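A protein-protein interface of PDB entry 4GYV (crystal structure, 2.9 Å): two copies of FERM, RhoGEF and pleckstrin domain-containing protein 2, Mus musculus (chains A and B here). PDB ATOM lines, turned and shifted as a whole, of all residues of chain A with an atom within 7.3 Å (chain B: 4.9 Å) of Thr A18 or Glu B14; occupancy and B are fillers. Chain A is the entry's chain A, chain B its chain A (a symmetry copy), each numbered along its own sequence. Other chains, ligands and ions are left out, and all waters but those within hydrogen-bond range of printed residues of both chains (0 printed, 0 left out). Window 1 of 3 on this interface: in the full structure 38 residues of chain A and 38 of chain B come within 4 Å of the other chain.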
ATOM      1  N   ILE A  11      24.790 -30.271 -12.613  1.00  0.00           N
ATOM      2  CA  ILE A  11      25.249 -29.051 -13.262  1.00  0.00           C
ATOM      3  C   ILE A  11      25.297 -29.255 -14.765  1.00  0.00           C
ATOM      4  O   ILE A  11      24.822 -28.416 -15.520  1.00  0.00           O
ATOM      5  CB  ILE A  11      26.619 -28.610 -12.748  1.00  0.00           C
ATOM      6  CG1 ILE A  11      26.534 -28.263 -11.281  1.00  0.00           C
ATOM      7  CG2 ILE A  11      27.132 -27.412 -13.522  1.00  0.00           C
ATOM      8  CD1 ILE A  11      27.890 -28.244 -10.632  1.00  0.00           C
ATOM      9  N   ALA A  12      25.836 -30.386 -15.195  1.00  0.00           N
ATOM     10  CA  ALA A  12      25.860 -30.722 -16.616  1.00  0.00           C
ATOM     11  C   ALA A  12      24.463 -30.650 -17.201  1.00  0.00           C
ATOM     12  O   ALA A  12      24.243 -30.027 -18.237  1.00  0.00           O
ATOM     13  CB  ALA A  12      26.439 -32.108 -16.834  1.00  0.00           C
ATOM     14  N   LYS A  13      23.509 -31.262 -16.518  1.00  0.00           N
ATOM     15  CA  LYS A  13      22.154 -31.281 -17.029  1.00  0.00           C
ATOM     16  C   LYS A  13      21.547 -29.871 -17.029  1.00  0.00           C
ATOM     17  O   LYS A  13      20.821 -29.503 -17.958  1.00  0.00           O
ATOM     18  CB  LYS A  13      21.305 -32.273 -16.252  1.00  0.00           C
ATOM     19  CG  LYS A  13      20.023 -32.587 -16.979  1.00  0.00           C
ATOM     20  CD  LYS A  13      20.026 -33.893 -17.776  1.00  0.00           C
ATOM     21  CE  LYS A  13      18.906 -33.850 -18.845  1.00  0.00           C
ATOM     22  NZ  LYS A  13      17.926 -34.988 -18.766  1.00  0.00           N
ATOM     23  N   GLU A  14      21.879 -29.077 -16.011  1.00  0.00           N
ATOM     24  CA  GLU A  14      21.443 -27.686 -15.941  1.00  0.00           C
ATOM     25  C   GLU A  14      22.027 -26.876 -17.114  1.00  0.00           C
ATOM     26  O   GLU A  14      21.340 -26.048 -17.712  1.00  0.00           O
ATOM     27  CB  GLU A  14      21.810 -27.051 -14.581  1.00  0.00           C
ATOM     28  CG  GLU A  14      20.952 -27.512 -13.369  1.00  0.00           C
ATOM     29  CD  GLU A  14      21.586 -27.198 -11.983  1.00  0.00           C
ATOM     30  OE1 GLU A  14      22.638 -26.515 -11.942  1.00  0.00           O
ATOM     31  OE2 GLU A  14      21.029 -27.619 -10.928  1.00  0.00           O
ATOM     32  N   ILE A  15      23.292 -27.122 -17.452  1.00  0.00           N
ATOM     33  CA  ILE A  15      23.908 -26.464 -18.600  1.00  0.00           C
ATOM     34  C   ILE A  15      23.151 -26.795 -19.883  1.00  0.00           C
ATOM     35  O   ILE A  15      22.806 -25.922 -20.674  1.00  0.00           O
ATOM     36  CB  ILE A  15      25.368 -26.886 -18.756  1.00  0.00           C
ATOM     37  CG1 ILE A  15      26.221 -26.313 -17.624  1.00  0.00           C
ATOM     38  CG2 ILE A  15      25.968 -26.405 -20.083  1.00  0.00           C
ATOM     39  CD1 ILE A  15      27.635 -26.868 -17.679  1.00  0.00           C
ATOM     40  N   LEU A  16      22.873 -28.069 -20.074  1.00  0.00           N
ATOM     41  CA  LEU A  16      22.173 -28.520 -21.259  1.00  0.00           C
ATOM     42  C   LEU A  16      20.770 -27.945 -21.362  1.00  0.00           C
ATOM     43  O   LEU A  16      20.422 -27.326 -22.354  1.00  0.00           O
ATOM     44  CB  LEU A  16      22.081 -30.034 -21.240  1.00  0.00           C
ATOM     45  CG  LEU A  16      21.333 -30.587 -22.439  1.00  0.00           C
ATOM     46  CD1 LEU A  16      22.105 -30.193 -23.645  1.00  0.00           C
ATOM     47  CD2 LEU A  16      21.244 -32.078 -22.373  1.00  0.00           C
ATOM     48  N   ALA A  17      19.959 -28.165 -20.341  1.00  0.00           N
ATOM     49  CA  ALA A  17      18.578 -27.712 -20.394  1.00  0.00           C
ATOM     50  C   ALA A  17      18.501 -26.214 -20.624  1.00  0.00           C
ATOM     51  O   ALA A  17      17.670 -25.745 -21.397  1.00  0.00           O
ATOM     52  CB  ALA A  17      17.832 -28.089 -19.128  1.00  0.00           C
ATOM     53  N   THR A  18      19.365 -25.460 -19.963  1.00  0.00           N
ATOM     54  CA  THR A  18      19.335 -24.023 -20.142  1.00  0.00           C
ATOM     55  C   THR A  18      19.888 -23.574 -21.497  1.00  0.00           C
ATOM     56  O   THR A  18      19.478 -22.547 -22.016  1.00  0.00           O
ATOM     57  CB  THR A  18      20.016 -23.260 -18.974  1.00  0.00           C
ATOM     58  OG1 THR A  18      21.406 -23.593 -18.901  1.00  0.00           O
ATOM     59  CG2 THR A  18      19.326 -23.573 -17.676  1.00  0.00           C
ATOM     60  N   GLU A  19      20.806 -24.339 -22.070  1.00  0.00           N
ATOM     61  CA  GLU A  19      21.301 -24.030 -23.416  1.00  0.00           C
ATOM     62  C   GLU A  19      20.205 -24.152 -24.492  1.00  0.00           C
ATOM     63  O   GLU A  19      20.081 -23.266 -25.344  1.00  0.00           O
ATOM     64  CB  GLU A  19      22.488 -24.918 -23.800  1.00  0.00           C
ATOM     65  CG  GLU A  19      23.232 -24.426 -25.029  1.00  0.00           C
ATOM     66  CD  GLU A  19      24.122 -23.195 -24.732  1.00  0.00           C
ATOM     67  OE1 GLU A  19      24.205 -22.758 -23.558  1.00  0.00           O
ATOM     68  OE2 GLU A  19      24.744 -22.664 -25.677  1.00  0.00           O
ATOM     69  N   ARG A  20      19.438 -25.250 -24.444  1.00  0.00           N
ATOM     70  CA  ARG A  20      18.334 -25.496 -25.369  1.00  0.00           C
ATOM     71  C   ARG A  20      17.346 -24.323 -25.373  1.00  0.00           C
ATOM     72  O   ARG A  20      16.970 -23.836 -26.435  1.00  0.00           O
ATOM     73  CB  ARG A  20      17.611 -26.808 -25.038  1.00  0.00           C
ATOM     74  CG  ARG A  20      17.762 -27.930 -26.068  1.00  0.00           C
ATOM     75  CD  ARG A  20      16.792 -29.106 -25.842  1.00  0.00           C
ATOM     76  NE  ARG A  20      17.469 -30.374 -25.510  1.00  0.00           N
ATOM     77  CZ  ARG A  20      17.481 -30.950 -24.301  1.00  0.00           C
ATOM     78  NH1 ARG A  20      16.855 -30.379 -23.276  1.00  0.00           N
ATOM     79  NH2 ARG A  20      18.119 -32.105 -24.115  1.00  0.00           N
ATOM     80  N   THR A  21      16.947 -23.858 -24.189  1.00  0.00           N
ATOM     81  CA  THR A  21      16.028 -22.737 -24.075  1.00  0.00           C
ATOM     82  C   THR A  21      16.611 -21.445 -24.637  1.00  0.00           C
ATOM     83  O   THR A  21      15.923 -20.683 -25.306  1.00  0.00           O
ATOM     84  CB  THR A  21      15.680 -22.442 -22.620  1.00  0.00           C
ATOM     85  OG1 THR A  21      15.080 -23.586 -22.045  1.00  0.00           O
ATOM     86  CG2 THR A  21      14.681 -21.292 -22.533  1.00  0.00           C
ATOM     87  N   TYR A  22      17.871 -21.174 -24.329  1.00  0.00           N
ATOM     88  CA  TYR A  22      18.463 -19.900 -24.707  1.00  0.00           C
ATOM     89  C   TYR A  22      18.505 -19.847 -26.219  1.00  0.00           C
ATOM     90  O   TYR A  22      18.299 -18.788 -26.817  1.00  0.00           O
ATOM     91  CB  TYR A  22      19.844 -19.732 -24.065  1.00  0.00           C
ATOM     92  CG  TYR A  22      20.787 -18.778 -24.745  1.00  0.00           C
ATOM     93  CD1 TYR A  22      20.635 -17.415 -24.620  1.00  0.00           C
ATOM     94  CD2 TYR A  22      21.853 -19.248 -25.492  1.00  0.00           C
ATOM     95  CE1 TYR A  22      21.509 -16.541 -25.246  1.00  0.00           C
ATOM     96  CE2 TYR A  22      22.729 -18.391 -26.119  1.00  0.00           C
ATOM     97  CZ  TYR A  22      22.551 -17.041 -25.995  1.00  0.00           C
ATOM     98  OH  TYR A  22      23.429 -16.185 -26.606  1.00  0.00           O
ATOM     99  N   LEU A  23      18.719 -21.009 -26.833  1.00  0.00           N
ATOM    100  CA  LEU A  23      18.735 -21.129 -28.287  1.00  0.00           C
ATOM    101  C   LEU A  23      17.386 -20.809 -28.914  1.00  0.00           C
ATOM    102  O   LEU A  23      17.306 -19.994 -29.837  1.00  0.00           O
ATOM    103  CB  LEU A  23      19.259 -22.499 -28.713  1.00  0.00           C
ATOM    104  CG  LEU A  23      20.789 -22.458 -28.733  1.00  0.00           C
ATOM    105  CD1 LEU A  23      21.380 -23.817 -28.668  1.00  0.00           C
ATOM    106  CD2 LEU A  23      21.309 -21.727 -29.951  1.00  0.00           C
ATOM    107  N   LYS A  24      16.328 -21.431 -28.403  1.00  0.00           N
ATOM    108  CA  LYS A  24      14.976 -21.104 -28.814  1.00  0.00           C
ATOM    109  C   LYS A  24      14.701 -19.586 -28.648  1.00  0.00           C
ATOM    110  O   LYS A  24      13.960 -19.000 -29.431  1.00  0.00           O
ATOM    111  CB  LYS A  24      13.972 -21.931 -28.013  1.00  0.00           C
ATOM    112  CG  LYS A  24      13.798 -23.378 -28.469  1.00  0.00           C
ATOM    113  CD  LYS A  24      12.363 -23.636 -28.992  1.00  0.00           C
ATOM    114  CE  LYS A  24      12.278 -24.861 -29.931  1.00  0.00           C
ATOM    115  NZ  LYS A  24      12.469 -26.177 -29.229  1.00  0.00           N
ATOM    116  N   ASP A  25      15.302 -18.957 -27.638  1.00  0.00           N
ATOM    117  CA  ASP A  25      15.127 -17.522 -27.413  1.00  0.00           C
ATOM    118  C   ASP A  25      15.815 -16.720 -28.517  1.00  0.00           C
ATOM    119  O   ASP A  25      15.229 -15.785 -29.064  1.00  0.00           O
ATOM    120  CB  ASP A  25      15.618 -17.097 -26.019  1.00  0.00           C
ATOM    121  CG  ASP A  25      14.645 -17.484 -24.905  1.00  0.00           C
ATOM    122  OD1 ASP A  25      13.452 -17.718 -25.223  1.00  0.00           O
ATOM    123  OD2 ASP A  25      15.065 -17.545 -23.717  1.00  0.00           O
ATOM    124  N   LEU A  66      25.828 -26.776 -28.056  1.00  0.00           N
ATOM    125  CA  LEU A  66      24.706 -27.585 -27.632  1.00  0.00           C
ATOM    126  C   LEU A  66      24.870 -28.979 -28.184  1.00  0.00           C
ATOM    127  O   LEU A  66      24.601 -29.966 -27.515  1.00  0.00           O
ATOM    128  CB  LEU A  66      23.390 -26.991 -28.121  1.00  0.00           C
ATOM    129  CG  LEU A  66      22.146 -27.868 -27.918  1.00  0.00           C
ATOM    130  CD1 LEU A  66      21.949 -28.161 -26.459  1.00  0.00           C
ATOM    131  CD2 LEU A  66      20.890 -27.213 -28.495  1.00  0.00           C
ATOM    132  N   ARG A 156      24.060 -14.899 -20.921  1.00  0.00           N
ATOM    133  CA  ARG A 156      24.376 -16.333 -21.003  1.00  0.00           C
ATOM    134  C   ARG A 156      25.823 -16.566 -20.620  1.00  0.00           C
ATOM    135  O   ARG A 156      26.147 -17.556 -19.967  1.00  0.00           O
ATOM    136  CB  ARG A 156      24.105 -16.900 -22.394  1.00  0.00           C
ATOM    137  CG  ARG A 156      24.284 -18.384 -22.533  1.00  0.00           C
ATOM    138  CD  ARG A 156      23.253 -19.157 -21.730  1.00  0.00           C
ATOM    139  NE  ARG A 156      23.474 -20.608 -21.815  1.00  0.00           N
ATOM    140  CZ  ARG A 156      23.131 -21.485 -20.872  1.00  0.00           C
ATOM    141  NH1 ARG A 156      22.553 -21.078 -19.756  1.00  0.00           N
ATOM    142  NH2 ARG A 156      23.372 -22.774 -21.043  1.00  0.00           N
ATOM    143  N   HIS A 159      26.135 -16.538 -16.903  1.00  0.00           N
ATOM    144  CA  HIS A 159      25.644 -17.828 -16.465  1.00  0.00           C
ATOM    145  C   HIS A 159      26.709 -18.906 -16.580  1.00  0.00           C
ATOM    146  O   HIS A 159      26.865 -19.695 -15.660  1.00  0.00           O
ATOM    147  CB  HIS A 159      24.409 -18.226 -17.268  1.00  0.00           C
ATOM    148  CG  HIS A 159      23.493 -19.158 -16.534  1.00  0.00           C
ATOM    149  ND1 HIS A 159      22.248 -19.510 -17.004  1.00  0.00           N
ATOM    150  CD2 HIS A 159      23.647 -19.816 -15.363  1.00  0.00           C
ATOM    151  CE1 HIS A 159      21.670 -20.335 -16.149  1.00  0.00           C
ATOM    152  NE2 HIS A 159      22.497 -20.532 -15.141  1.00  0.00           N
ATOM    153  N   TYR A 160      27.438 -18.938 -17.701  1.00  0.00           N
ATOM    154  CA  TYR A 160      28.534 -19.896 -17.878  1.00  0.00           C
ATOM    155  C   TYR A 160      29.566 -19.769 -16.750  1.00  0.00           C
ATOM    156  O   TYR A 160      30.004 -20.777 -16.182  1.00  0.00           O
ATOM    157  CB  TYR A 160      29.247 -19.713 -19.220  1.00  0.00           C
ATOM    158  CG  TYR A 160      28.489 -20.183 -20.457  1.00  0.00           C
ATOM    159  CD1 TYR A 160      27.351 -20.995 -20.363  1.00  0.00           C
ATOM    160  CD2 TYR A 160      28.920 -19.815 -21.732  1.00  0.00           C
ATOM    161  CE1 TYR A 160      26.663 -21.417 -21.517  1.00  0.00           C
ATOM    162  CE2 TYR A 160      28.247 -20.233 -22.879  1.00  0.00           C
ATOM    163  CZ  TYR A 160      27.128 -21.028 -22.764  1.00  0.00           C
ATOM    164  OH  TYR A 160      26.483 -21.421 -23.912  1.00  0.00           O
ATOM    165  N   LEU A 162      29.145 -18.770 -13.878  1.00  0.00           N
ATOM    166  CA  LEU A 162      28.518 -19.197 -12.643  1.00  0.00           C
ATOM    167  C   LEU A 162      28.570 -20.696 -12.525  1.00  0.00           C
ATOM    168  O   LEU A 162      28.976 -21.236 -11.493  1.00  0.00           O
ATOM    169  CB  LEU A 162      27.063 -18.774 -12.657  1.00  0.00           C
ATOM    170  CG  LEU A 162      26.697 -17.652 -11.721  1.00  0.00           C
ATOM    171  CD1 LEU A 162      26.652 -18.273 -10.333  1.00  0.00           C
ATOM    172  CD2 LEU A 162      27.741 -16.504 -11.851  1.00  0.00           C
ATOM    173  N   LEU A 163      28.131 -21.351 -13.603  1.00  0.00           N
ATOM    174  CA  LEU A 163      28.073 -22.801 -13.716  1.00  0.00           C
ATOM    175  C   LEU A 163      29.452 -23.445 -13.586  1.00  0.00           C
ATOM    176  O   LEU A 163      29.622 -24.402 -12.841  1.00  0.00           O
ATOM    177  CB  LEU A 163      27.399 -23.191 -15.034  1.00  0.00           C
ATOM    178  CG  LEU A 163      25.893 -22.894 -15.114  1.00  0.00           C
ATOM    179  CD1 LEU A 163      25.457 -22.609 -16.541  1.00  0.00           C
ATOM    180  CD2 LEU A 163      25.043 -24.017 -14.506  1.00  0.00           C
ATOM    181  N   ARG A 166      30.601 -23.527 -10.055  1.00  0.00           N
ATOM    182  CA  ARG A 166      30.022 -24.535  -9.193  1.00  0.00           C
ATOM    183  C   ARG A 166      30.741 -25.860  -9.380  1.00  0.00           C
ATOM    184  O   ARG A 166      31.017 -26.578  -8.404  1.00  0.00           O
ATOM    185  CB  ARG A 166      28.554 -24.698  -9.504  1.00  0.00           C
ATOM    186  CG  ARG A 166      27.795 -23.401  -9.598  1.00  0.00           C
ATOM    187  CD  ARG A 166      26.502 -23.467  -8.799  1.00  0.00           C
ATOM    188  NE  ARG A 166      25.736 -24.676  -9.090  1.00  0.00           N
ATOM    189  CZ  ARG A 166      24.901 -24.795 -10.113  1.00  0.00           C
ATOM    190  NH1 ARG A 166      24.707 -23.761 -10.951  1.00  0.00           N
ATOM    191  NH2 ARG A 166      24.250 -25.943 -10.277  1.00  0.00           N
ATOM    192  N   PHE B  10      18.967 -16.986 -12.116  1.00  0.00           N
ATOM    193  CA  PHE B  10      19.546 -18.172 -12.752  1.00  0.00           C
ATOM    194  C   PHE B  10      19.047 -19.491 -12.167  1.00  0.00           C
ATOM    195  O   PHE B  10      18.720 -20.406 -12.899  1.00  0.00           O
ATOM    196  CB  PHE B  10      21.062 -18.128 -12.747  1.00  0.00           C
ATOM    197  CG  PHE B  10      21.641 -17.025 -13.595  1.00  0.00           C
ATOM    198  CD1 PHE B  10      21.348 -16.941 -14.945  1.00  0.00           C
ATOM    199  CD2 PHE B  10      22.508 -16.082 -13.048  1.00  0.00           C
ATOM    200  CE1 PHE B  10      21.888 -15.925 -15.734  1.00  0.00           C
ATOM    201  CE2 PHE B  10      23.055 -15.072 -13.832  1.00  0.00           C
ATOM    202  CZ  PHE B  10      22.737 -14.986 -15.172  1.00  0.00           C
ATOM    203  N   ILE B  11      18.958 -19.595 -10.852  1.00  0.00           N
ATOM    204  CA  ILE B  11      18.459 -20.828 -10.258  1.00  0.00           C
ATOM    205  C   ILE B  11      17.025 -21.063 -10.690  1.00  0.00           C
ATOM    206  O   ILE B  11      16.670 -22.164 -11.092  1.00  0.00           O
ATOM    207  CB  ILE B  11      18.552 -20.806  -8.733  1.00  0.00           C
ATOM    208  CG1 ILE B  11      19.997 -20.724  -8.303  1.00  0.00           C
ATOM    209  CG2 ILE B  11      17.916 -22.044  -8.130  1.00  0.00           C
ATOM    210  CD1 ILE B  11      20.129 -20.272  -6.875  1.00  0.00           C
ATOM    211  N   ALA B  12      16.210 -20.020 -10.643  1.00  0.00           N
ATOM    212  CA  ALA B  12      14.831 -20.111 -11.113  1.00  0.00           C
ATOM    213  C   ALA B  12      14.789 -20.638 -12.534  1.00  0.00           C
ATOM    214  O   ALA B  12      14.045 -21.566 -12.843  1.00  0.00           O
ATOM    215  CB  ALA B  12      14.144 -18.760 -11.045  1.00  0.00           C
ATOM    216  N   LYS B  13      15.615 -20.066 -13.396  1.00  0.00           N
ATOM    217  CA  LYS B  13      15.608 -20.478 -14.784  1.00  0.00           C
ATOM    218  C   LYS B  13      16.110 -21.922 -14.932  1.00  0.00           C
ATOM    219  O   LYS B  13      15.584 -22.685 -15.748  1.00  0.00           O
ATOM    220  CB  LYS B  13      16.406 -19.502 -15.634  1.00  0.00           C
ATOM    221  CG  LYS B  13      16.114 -19.686 -17.101  1.00  0.00           C
ATOM    222  CD  LYS B  13      15.112 -18.696 -17.698  1.00  0.00           C
ATOM    223  CE  LYS B  13      14.526 -19.277 -19.007  1.00  0.00           C
ATOM    224  NZ  LYS B  13      14.698 -18.395 -20.213  1.00  0.00           N
ATOM    225  N   GLU B  14      17.093 -22.300 -14.116  1.00  0.00           N
ATOM    226  CA  GLU B  14      17.595 -23.670 -14.093  1.00  0.00           C
ATOM    227  C   GLU B  14      16.489 -24.645 -13.649  1.00  0.00           C
ATOM    228  O   GLU B  14      16.349 -25.734 -14.204  1.00  0.00           O
ATOM    229  CB  GLU B  14      18.848 -23.793 -13.195  1.00  0.00           C
ATOM    230  CG  GLU B  14      20.156 -23.190 -13.778  1.00  0.00           C
ATOM    231  CD  GLU B  14      21.273 -22.949 -12.722  1.00  0.00           C
ATOM    232  OE1 GLU B  14      21.092 -23.357 -11.548  1.00  0.00           O
ATOM    233  OE2 GLU B  14      22.343 -22.366 -13.061  1.00  0.00           O
ATOM    234  N   ILE B  15      15.694 -24.250 -12.655  1.00  0.00           N
ATOM    235  CA  ILE B  15      14.568 -25.069 -12.219  1.00  0.00           C
ATOM    236  C   ILE B  15      13.583 -25.290 -13.364  1.00  0.00           C
ATOM    237  O   ILE B  15      13.158 -26.405 -13.647  1.00  0.00           O
ATOM    238  CB  ILE B  15      13.836 -24.417 -11.047  1.00  0.00           C
ATOM    239  CG1 ILE B  15      14.698 -24.448  -9.785  1.00  0.00           C
ATOM    240  CG2 ILE B  15      12.514 -25.127 -10.726  1.00  0.00           C
ATOM    241  CD1 ILE B  15      14.048 -23.652  -8.666  1.00  0.00           C
ATOM    242  N   LEU B  16      13.239 -24.211 -14.041  1.00  0.00           N
ATOM    243  CA  LEU B  16      12.300 -24.279 -15.142  1.00  0.00           C
ATOM    244  C   LEU B  16      12.806 -25.137 -16.289  1.00  0.00           C
ATOM    245  O   LEU B  16      12.146 -26.075 -16.704  1.00  0.00           O
ATOM    246  CB  LEU B  16      12.035 -22.878 -15.659  1.00  0.00           C
ATOM    247  CG  LEU B  16      11.078 -22.863 -16.838  1.00  0.00           C
ATOM    248  CD1 LEU B  16       9.791 -23.421 -16.351  1.00  0.00           C
ATOM    249  CD2 LEU B  16      10.860 -21.470 -17.332  1.00  0.00           C
ATOM    250  N   ALA B  17      13.974 -24.804 -16.812  1.00  0.00           N
ATOM    251  CA  ALA B  17      14.494 -25.530 -17.960  1.00  0.00           C
ATOM    252  C   ALA B  17      14.621 -27.012 -17.662  1.00  0.00           C
ATOM    253  O   ALA B  17      14.295 -27.846 -18.502  1.00  0.00           O
ATOM    254  CB  ALA B  17      15.832 -24.966 -18.402  1.00  0.00           C
ATOM    255  N   THR B  18      15.086 -27.346 -16.468  1.00  0.00           N
ATOM    256  CA  THR B  18      15.231 -28.746 -16.129  1.00  0.00           C
ATOM    257  C   THR B  18      13.894 -29.443 -15.868  1.00  0.00           C
ATOM    258  O   THR B  18      13.772 -30.638 -16.090  1.00  0.00           O
ATOM    259  CB  THR B  18      16.226 -28.980 -14.960  1.00  0.00           C
ATOM    260  OG1 THR B  18      15.746 -28.360 -13.762  1.00  0.00           O
ATOM    261  CG2 THR B  18      17.586 -28.455 -15.323  1.00  0.00           C
ATOM    262  N   GLU B  19      12.894 -28.704 -15.408  1.00  0.00           N
ATOM    263  CA  GLU B  19      11.556 -29.279 -15.239  1.00  0.00           C
ATOM    264  C   GLU B  19      10.921 -29.705 -16.577  1.00  0.00           C
ATOM    265  O   GLU B  19      10.367 -30.805 -16.671  1.00  0.00           O
ATOM    266  CB  GLU B  19      10.613 -28.315 -14.515  1.00  0.00           C
ATOM    267  CG  GLU B  19       9.334 -28.976 -14.032  1.00  0.00           C
ATOM    268  CD  GLU B  19       9.556 -29.855 -12.779  1.00  0.00           C
ATOM    269  OE1 GLU B  19      10.693 -29.906 -12.250  1.00  0.00           O
ATOM    270  OE2 GLU B  19       8.586 -30.496 -12.317  1.00  0.00           O
ATOM    271  N   LEU B 163      18.757 -27.523  -5.483  1.00  0.00           N
ATOM    272  CA  LEU B 163      18.372 -26.213  -5.987  1.00  0.00           C
ATOM    273  C   LEU B 163      17.884 -25.287  -4.874  1.00  0.00           C
ATOM    274  O   LEU B 163      18.309 -24.142  -4.789  1.00  0.00           O
ATOM    275  CB  LEU B 163      17.316 -26.370  -7.083  1.00  0.00           C
ATOM    276  CG  LEU B 163      17.820 -26.984  -8.400  1.00  0.00           C
ATOM    277  CD1 LEU B 163      16.723 -27.754  -9.112  1.00  0.00           C
ATOM    278  CD2 LEU B 163      18.436 -25.935  -9.334  1.00  0.00           C
ATOM    279  N   ARG B 166      20.707 -23.951  -2.865  1.00  0.00           N
ATOM    280  CA  ARG B 166      21.487 -22.878  -3.448  1.00  0.00           C
ATOM    281  C   ARG B 166      20.793 -21.546  -3.226  1.00  0.00           C
ATOM    282  O   ARG B 166      21.443 -20.534  -2.910  1.00  0.00           O
ATOM    283  CB  ARG B 166      21.671 -23.121  -4.927  1.00  0.00           C
ATOM    284  CG  ARG B 166      22.115 -24.518  -5.273  1.00  0.00           C
ATOM    285  CD  ARG B 166      23.277 -24.493  -6.254  1.00  0.00           C
ATOM    286  NE  ARG B 166      23.023 -23.606  -7.386  1.00  0.00           N
ATOM    287  CZ  ARG B 166      22.347 -23.966  -8.469  1.00  0.00           C
ATOM    288  NH1 ARG B 166      21.861 -25.214  -8.581  1.00  0.00           N
ATOM    289  NH2 ARG B 166      22.183 -23.075  -9.444  1.00  0.00           N
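Of the 12 printed residues of chain B, 7 touch a printed residue of chain A.
Hydrophobic or aromatic side chains of chain B within 4 Å of the printed part of chain A: Phe B10, Ala B17 and Leu B163.
Hydrophobic or aromatic side chains of chain A within 4 Å of the printed part of chain B: Ala A17, His A159 and Leu A163.
Among the printed residues, 16 pairs touch across the chains.
Among the printed residues, Asp or Glu carboxylates within 4 Å of a Lys or Arg side-chain nitrogen of the other chain: Glu A14 with Arg B166 (3.5 Å), Asp A25 with Lys B13 (3.6 Å) and Arg A166 with Glu B14 (3.5 Å).
Glu A14 touches its own counterpart, Glu B14.
Ala A17 touches its own counterpart, Ala B17.
Ala A17 touches Thr B18, and with the chains exchanged Thr A18 touches Ala B17.
Arg B166 touches its own counterpart, Arg A166.
Of the 16 pairs that touch across the chains among the printed residues, 11 have their exchanged pair printed and touching as well.
Among the printed residues, pairs that only touch across the chains: Glu A14 with Glu B14, Glu A14 with Thr B18, Glu A14 with Leu B163, Ala A17 with Ala B17, Ala A17 with Thr B18, Thr A18 with Glu B14, Thr A18 with Ala B17, Thr A21 with Lys B13, Thr A21 with Ala B17, His A159 with Phe B10 and Leu A163 with Glu B14.
OE2 of Glu A14 is in salt-bridge range of NH1 of Arg B166 (3.5 Å).
NZ of Lys B13 lies within salt-bridge range of OD2 of Asp A25, 3.6 Å away.
A ring nitrogen (NE2) of His A159 sits at hydrogen-bond distance from the side-chain carboxylate of Glu B14, 2.8 Å away.
NH1 of Arg A166 lies within salt-bridge range of OE2 of Glu B14 (3.5 Å).
NH1 of Arg A166 sits close to NH2 of Arg B166, 3.0 Å away.
Printed residues of chain B within 4 Å of Glu A14: Glu B14, Thr B18, Leu B163 and Arg B166.
Ile A15 touches none of the printed residues of chain B.
Printed residues of chain B within 4 Å of Thr A18: Glu B14 (3.98 Å) and Ala B17 (3.8 Å).
Of the printed residues of chain B, Arg A166 touches Glu B14 and Arg B166.
Of the printed residues of chain A, Lys B13 touches Thr A21 and Asp A25.
Printed residues of chain A within 4 Å of Glu B14: Glu A14 (3.5 Å), Thr A18 (3.98 Å), His A159 (2.8 Å), Leu A163 (3.5 Å) and Arg A166 (3.5 Å).
Of the printed residues of chain A, Ala B17 touches Ala A17, Thr A18 and Thr A21.
Printed residues of chain A within 4 Å of Thr B18: Glu A14 and Ala A17.
The nearest printed residue of chain B that does not touch Thr A18 is Lys B13 (4.3 Å).
The nearest printed residue of chain A that does not touch Glu B14 is Ala A17 (5.7 Å).
The nearest printed residue of chain A that does not touch Lys B13 is Thr A18 (4.3 Å).
The side-chain hydroxyl of Thr A18 sits at hydrogen-bond distance from the backbone carbonyl oxygen of Glu A14, at 2.7 Å.
NH1 of Arg A166 lies within salt-bridge range of OE1 of Glu A14, at 3.6 Å.
O of Ala A17 is in hydrogen-bond range of OG1 of Thr A21 (3.4 Å).
The guanidinium group (NH1) of Arg A156 is in hydrogen-bond range of the side-chain hydroxyl (OG1) of Thr A18, 2.9 Å away.
OG1 of Thr B18 lies within hydrogen-bond range of O of Glu B14 (2.7 Å).
The side-chain carboxylate (OE1) of Glu B14 lies within salt-bridge range of the guanidinium group (NH1) of Arg B166.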
